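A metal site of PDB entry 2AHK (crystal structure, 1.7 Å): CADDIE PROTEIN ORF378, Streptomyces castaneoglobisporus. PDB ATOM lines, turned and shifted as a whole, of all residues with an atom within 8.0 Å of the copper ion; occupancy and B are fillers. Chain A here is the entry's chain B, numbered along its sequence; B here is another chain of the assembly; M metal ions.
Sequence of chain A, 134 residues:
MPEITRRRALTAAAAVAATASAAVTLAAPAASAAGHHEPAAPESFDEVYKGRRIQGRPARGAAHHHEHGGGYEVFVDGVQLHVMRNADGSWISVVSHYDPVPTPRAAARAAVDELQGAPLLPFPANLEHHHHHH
NE2 of His 97 is bound to the copper ion, 2.2 Å away.
NE2 of His 82 is bound to the copper ion, at 2.2 Å.
SD of Met 84 binds the copper ion (2.5 Å).
The copper ion has three donor atoms within binding distance.
Merely in contact with the copper ion: Ile 42 of chain B and Met 43 of chain B.
Of the 19 residues printed, 5 come within 4 Å of the copper ion.
A ring nitrogen (NE2) of His 97 sits close to the backbone carbonyl oxygen (O) of Ile 42 of chain B (3.4 Å).
The backbone carbonyl oxygen (O) of His 82 lies within hydrogen-bond range of the backbone NH (N) of Val 94 (2.9 Å).
The backbone carbonyl oxygen (O) of Ile 92 lies within hydrogen-bond range of the backbone NH (N) of Met 84 (2.8 Å).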
ATOM      1  N   HIS A  82      11.921   5.740 -23.494  1.00  0.00           N
ATOM      2  CA  HIS A  82      11.764   4.358 -23.928  1.00  0.00           C
ATOM      3  C   HIS A  82      12.890   4.019 -24.882  1.00  0.00           C
ATOM      4  O   HIS A  82      13.126   4.730 -25.852  1.00  0.00           O
ATOM      5  CB  HIS A  82      10.414   4.149 -24.620  1.00  0.00           C
ATOM      6  CG  HIS A  82      10.328   2.868 -25.380  1.00  0.00           C
ATOM      7  ND1 HIS A  82      10.073   1.663 -24.777  1.00  0.00           N
ATOM      8  CD2 HIS A  82      10.459   2.610 -26.705  1.00  0.00           C
ATOM      9  CE1 HIS A  82      10.059   0.705 -25.684  1.00  0.00           C
ATOM     10  NE2 HIS A  82      10.286   1.251 -26.868  1.00  0.00           N
ATOM     11  N   VAL A  83      13.608   2.936 -24.574  1.00  0.00           N
ATOM     12  CA  VAL A  83      14.709   2.487 -25.409  1.00  0.00           C
ATOM     13  C   VAL A  83      14.545   0.980 -25.593  1.00  0.00           C
ATOM     14  O   VAL A  83      13.921   0.317 -24.756  1.00  0.00           O
ATOM     15  CB  VAL A  83      16.108   2.802 -24.759  1.00  0.00           C
ATOM     16  CG1 VAL A  83      16.302   4.316 -24.653  1.00  0.00           C
ATOM     17  CG2 VAL A  83      16.207   2.171 -23.387  1.00  0.00           C
ATOM     18  N   MET A  84      15.096   0.447 -26.683  1.00  0.00           N
ATOM     19  CA  MET A  84      14.991  -0.979 -26.959  1.00  0.00           C
ATOM     20  C   MET A  84      16.306  -1.526 -27.503  1.00  0.00           C
ATOM     21  O   MET A  84      17.041  -0.813 -28.185  1.00  0.00           O
ATOM     22  CB  MET A  84      13.886  -1.260 -27.972  1.00  0.00           C
ATOM     23  CG  MET A  84      12.708  -2.045 -27.426  1.00  0.00           C
ATOM     24  SD  MET A  84      11.313  -2.094 -28.593  1.00  0.00           S
ATOM     25  CE  MET A  84      12.122  -2.838 -30.027  1.00  0.00           C
ATOM     26  N   ARG A  85      16.590  -2.774 -27.193  1.00  0.00           N
ATOM     27  CA  ARG A  85      17.818  -3.401 -27.676  1.00  0.00           C
ATOM     28  C   ARG A  85      17.504  -4.335 -28.845  1.00  0.00           C
ATOM     29  O   ARG A  85      16.597  -5.157 -28.770  1.00  0.00           O
ATOM     30  CB  ARG A  85      18.489  -4.194 -26.558  1.00  0.00           C
ATOM     31  CG  ARG A  85      19.833  -4.766 -26.987  1.00  0.00           C
ATOM     32  CD  ARG A  85      20.339  -5.794 -25.990  1.00  0.00           C
ATOM     33  NE  ARG A  85      21.609  -6.371 -26.430  1.00  0.00           N
ATOM     34  CZ  ARG A  85      21.716  -7.461 -27.186  1.00  0.00           C
ATOM     35  NH1 ARG A  85      20.616  -8.106 -27.587  1.00  0.00           N
ATOM     36  NH2 ARG A  85      22.914  -7.903 -27.558  1.00  0.00           N
ATOM     37  N   ASN A  86      18.282  -4.191 -29.908  1.00  0.00           N
ATOM     38  CA  ASN A  86      18.108  -5.012 -31.102  1.00  0.00           C
ATOM     39  C   ASN A  86      18.855  -6.318 -30.933  1.00  0.00           C
ATOM     40  O   ASN A  86      19.769  -6.405 -30.099  1.00  0.00           O
ATOM     41  CB  ASN A  86      18.611  -4.271 -32.327  1.00  0.00           C
ATOM     42  CG  ASN A  86      17.817  -3.023 -32.615  1.00  0.00           C
ATOM     43  OD1 ASN A  86      16.584  -3.077 -32.692  1.00  0.00           O
ATOM     44  ND2 ASN A  86      18.491  -1.900 -32.773  1.00  0.00           N
ATOM     45  N   ILE A  92      17.857   1.527 -29.948  1.00  0.00           N
ATOM     46  CA  ILE A  92      17.021   2.559 -30.550  1.00  0.00           C
ATOM     47  C   ILE A  92      16.175   3.108 -29.419  1.00  0.00           C
ATOM     48  O   ILE A  92      15.982   2.448 -28.406  1.00  0.00           O
ATOM     49  CB  ILE A  92      16.051   2.015 -31.620  1.00  0.00           C
ATOM     50  CG1 ILE A  92      15.296   0.805 -31.075  1.00  0.00           C
ATOM     51  CG2 ILE A  92      16.807   1.685 -32.905  1.00  0.00           C
ATOM     52  CD1 ILE A  92      14.390   0.173 -32.085  1.00  0.00           C
ATOM     53  N   SER A  93      15.690   4.331 -29.580  1.00  0.00           N
ATOM     54  CA  SER A  93      14.820   4.946 -28.584  1.00  0.00           C
ATOM     55  C   SER A  93      13.527   5.296 -29.300  1.00  0.00           C
ATOM     56  O   SER A  93      13.427   5.141 -30.524  1.00  0.00           O
ATOM     57  CB  SER A  93      15.456   6.206 -27.998  1.00  0.00           C
ATOM     58  OG  SER A  93      15.008   7.372 -28.675  1.00  0.00           O
ATOM     59  N   VAL A  94      12.538   5.748 -28.557  1.00  0.00           N
ATOM     60  CA  VAL A  94      11.267   6.114 -29.148  1.00  0.00           C
ATOM     61  C   VAL A  94      11.386   7.346 -30.051  1.00  0.00           C
ATOM     62  O   VAL A  94      10.599   7.495 -30.997  1.00  0.00           O
ATOM     63  CB  VAL A  94      10.188   6.329 -28.044  1.00  0.00           C
ATOM     64  CG1 VAL A  94      10.392   7.670 -27.360  1.00  0.00           C
ATOM     65  CG2 VAL A  94       8.797   6.203 -28.642  1.00  0.00           C
ATOM     66  N   HIS A  97      13.314   5.570 -33.524  1.00  0.00           N
ATOM     67  CA  HIS A  97      12.995   4.157 -33.598  1.00  0.00           C
ATOM     68  C   HIS A  97      13.291   3.386 -34.879  1.00  0.00           C
ATOM     69  O   HIS A  97      12.914   2.226 -34.985  1.00  0.00           O
ATOM     70  CB  HIS A  97      11.534   3.958 -33.243  1.00  0.00           C
ATOM     71  CG  HIS A  97      11.296   2.809 -32.323  1.00  0.00           C
ATOM     72  ND1 HIS A  97      11.471   1.496 -32.707  1.00  0.00           N
ATOM     73  CD2 HIS A  97      10.915   2.768 -31.024  1.00  0.00           C
ATOM     74  CE1 HIS A  97      11.201   0.696 -31.688  1.00  0.00           C
ATOM     75  NE2 HIS A  97      10.858   1.449 -30.652  1.00  0.00           N
ATOM     76  N   ASN B  39       2.351   3.637 -32.321  1.00  0.00           N
ATOM     77  CA  ASN B  39       3.350   3.846 -31.270  1.00  0.00           C
ATOM     78  C   ASN B  39       3.335   2.707 -30.259  1.00  0.00           C
ATOM     79  O   ASN B  39       4.383   2.173 -29.887  1.00  0.00           O
ATOM     80  CB  ASN B  39       3.111   5.183 -30.560  1.00  0.00           C
ATOM     81  CG  ASN B  39       4.275   5.588 -29.667  1.00  0.00           C
ATOM     82  OD1 ASN B  39       5.449   5.451 -30.047  1.00  0.00           O
ATOM     83  ND2 ASN B  39       3.967   6.096 -28.477  1.00  0.00           N
ATOM     84  N   GLU B  40       2.130   2.346 -29.804  1.00  0.00           N
ATOM     85  CA  GLU B  40       1.987   1.277 -28.827  1.00  0.00           C
ATOM     86  C   GLU B  40       2.599  -0.027 -29.311  1.00  0.00           C
ATOM     87  O   GLU B  40       3.239  -0.743 -28.532  1.00  0.00           O
ATOM     88  CB  GLU B  40       0.499   1.053 -28.519  1.00  0.00           C
ATOM     89  CG  GLU B  40      -0.056   2.004 -27.466  1.00  0.00           C
ATOM     90  CD  GLU B  40      -1.567   1.940 -27.358  1.00  0.00           C
ATOM     91  OE1 GLU B  40      -2.161   0.949 -27.854  1.00  0.00           O
ATOM     92  OE2 GLU B  40      -2.167   2.866 -26.771  1.00  0.00           O
ATOM     93  N   PHE B  41       2.420  -0.331 -30.596  1.00  0.00           N
ATOM     94  CA  PHE B  41       2.978  -1.566 -31.146  1.00  0.00           C
ATOM     95  C   PHE B  41       4.468  -1.473 -31.384  1.00  0.00           C
ATOM     96  O   PHE B  41       5.190  -2.439 -31.141  1.00  0.00           O
ATOM     97  CB  PHE B  41       2.262  -1.941 -32.448  1.00  0.00           C
ATOM     98  CG  PHE B  41       1.086  -2.843 -32.234  1.00  0.00           C
ATOM     99  CD1 PHE B  41       1.235  -4.228 -32.319  1.00  0.00           C
ATOM    100  CD2 PHE B  41      -0.160  -2.319 -31.908  1.00  0.00           C
ATOM    101  CE1 PHE B  41       0.162  -5.084 -32.089  1.00  0.00           C
ATOM    102  CE2 PHE B  41      -1.239  -3.157 -31.662  1.00  0.00           C
ATOM    103  CZ  PHE B  41      -1.087  -4.547 -31.761  1.00  0.00           C
ATOM    104  N   ILE B  42       4.941  -0.332 -31.858  1.00  0.00           N
ATOM    105  CA  ILE B  42       6.353  -0.161 -32.119  1.00  0.00           C
ATOM    106  C   ILE B  42       7.121  -0.248 -30.806  1.00  0.00           C
ATOM    107  O   ILE B  42       8.262  -0.705 -30.761  1.00  0.00           O
ATOM    108  CB  ILE B  42       6.625   1.192 -32.854  1.00  0.00           C
ATOM    109  CG1 ILE B  42       7.954   1.100 -33.602  1.00  0.00           C
ATOM    110  CG2 ILE B  42       6.603   2.356 -31.874  1.00  0.00           C
ATOM    111  CD1 ILE B  42       8.035   2.011 -34.801  1.00  0.00           C
ATOM    112  N   MET B  43       6.474   0.166 -29.722  1.00  0.00           N
ATOM    113  CA  MET B  43       7.094   0.121 -28.396  1.00  0.00           C
ATOM    114  C   MET B  43       7.050  -1.260 -27.740  1.00  0.00           C
ATOM    115  O   MET B  43       7.796  -1.526 -26.801  1.00  0.00           O
ATOM    116  CB  MET B  43       6.442   1.146 -27.478  1.00  0.00           C
ATOM    117  CG  MET B  43       6.888   2.577 -27.743  1.00  0.00           C
ATOM    118  SD  MET B  43       6.383   3.698 -26.428  1.00  0.00           S
ATOM    119  CE  MET B  43       4.662   3.219 -26.246  1.00  0.00           C
ATOM    120  N   SER B  44       6.180  -2.146 -28.225  1.00  0.00           N
ATOM    121  CA  SER B  44       6.076  -3.479 -27.648  1.00  0.00           C
ATOM    122  C   SER B  44       6.684  -4.608 -28.492  1.00  0.00           C
ATOM    123  O   SER B  44       7.016  -5.669 -27.972  1.00  0.00           O
ATOM    124  CB  SER B  44       4.602  -3.795 -27.345  1.00  0.00           C
ATOM    125  OG  SER B  44       3.912  -4.224 -28.500  1.00  0.00           O
ATOM    126  N   ASP B  45       6.838  -4.387 -29.804  1.00  0.00           N
ATOM    127  CA  ASP B  45       7.437  -5.377 -30.694  1.00  0.00           C
ATOM    128  C   ASP B  45       8.930  -5.491 -30.376  1.00  0.00           C
ATOM    129  O   ASP B  45       9.677  -4.536 -30.608  1.00  0.00           O
ATOM    130  CB  ASP B  45       7.278  -4.958 -32.164  1.00  0.00           C
ATOM    131  CG  ASP B  45       5.835  -4.991 -32.652  1.00  0.00           C
ATOM    132  OD1 ASP B  45       5.471  -4.117 -33.476  1.00  0.00           O
ATOM    133  OD2 ASP B  45       5.066  -5.881 -32.217  1.00  0.00           O
ATOM    134  N   THR B  46       9.364  -6.635 -29.855  1.00  0.00           N
ATOM    135  CA  THR B  46      10.772  -6.812 -29.520  1.00  0.00           C
ATOM    136  C   THR B  46      11.371  -8.089 -30.115  1.00  0.00           C
ATOM    137  O   THR B  46      10.672  -9.082 -30.303  1.00  0.00           O
ATOM    138  CB  THR B  46      10.988  -6.826 -28.004  1.00  0.00           C
ATOM    139  OG1 THR B  46      10.342  -7.969 -27.433  1.00  0.00           O
ATOM    140  CG2 THR B  46      10.413  -5.559 -27.376  1.00  0.00           C
ATOM    141  N   ARG B  55       9.880  -5.733 -36.939  1.00  0.00           N
ATOM    142  CA  ARG B  55      10.970  -6.690 -36.755  1.00  0.00           C
ATOM    143  C   ARG B  55      10.475  -8.130 -36.679  1.00  0.00           C
ATOM    144  O   ARG B  55      10.954  -8.921 -35.862  1.00  0.00           O
ATOM    145  CB  ARG B  55      11.772  -6.348 -35.494  1.00  0.00           C
ATOM    146  CG  ARG B  55      10.931  -6.059 -34.275  1.00  0.00           C
ATOM    147  CD  ARG B  55      11.781  -5.582 -33.096  1.00  0.00           C
ATOM    148  NE  ARG B  55      12.276  -4.228 -33.292  1.00  0.00           N
ATOM    149  CZ  ARG B  55      13.505  -3.825 -32.986  1.00  0.00           C
ATOM    150  NH1 ARG B  55      14.364  -4.695 -32.473  1.00  0.00           N
ATOM    151  NH2 ARG B  55      13.866  -2.569 -33.190  1.00  0.00           N
ATOM    152  N   GLY B 204       8.537   6.864 -32.976  1.00  0.00           N
ATOM    153  CA  GLY B 204       7.486   5.865 -32.849  1.00  0.00           C
ATOM    154  C   GLY B 204       6.117   6.398 -33.236  1.00  0.00           C
ATOM    155  O   GLY B 204       5.235   5.638 -33.624  1.00  0.00           O
HETATM  156 CU    CU M   1      10.850   0.306 -28.778  1.00  0.00          CU
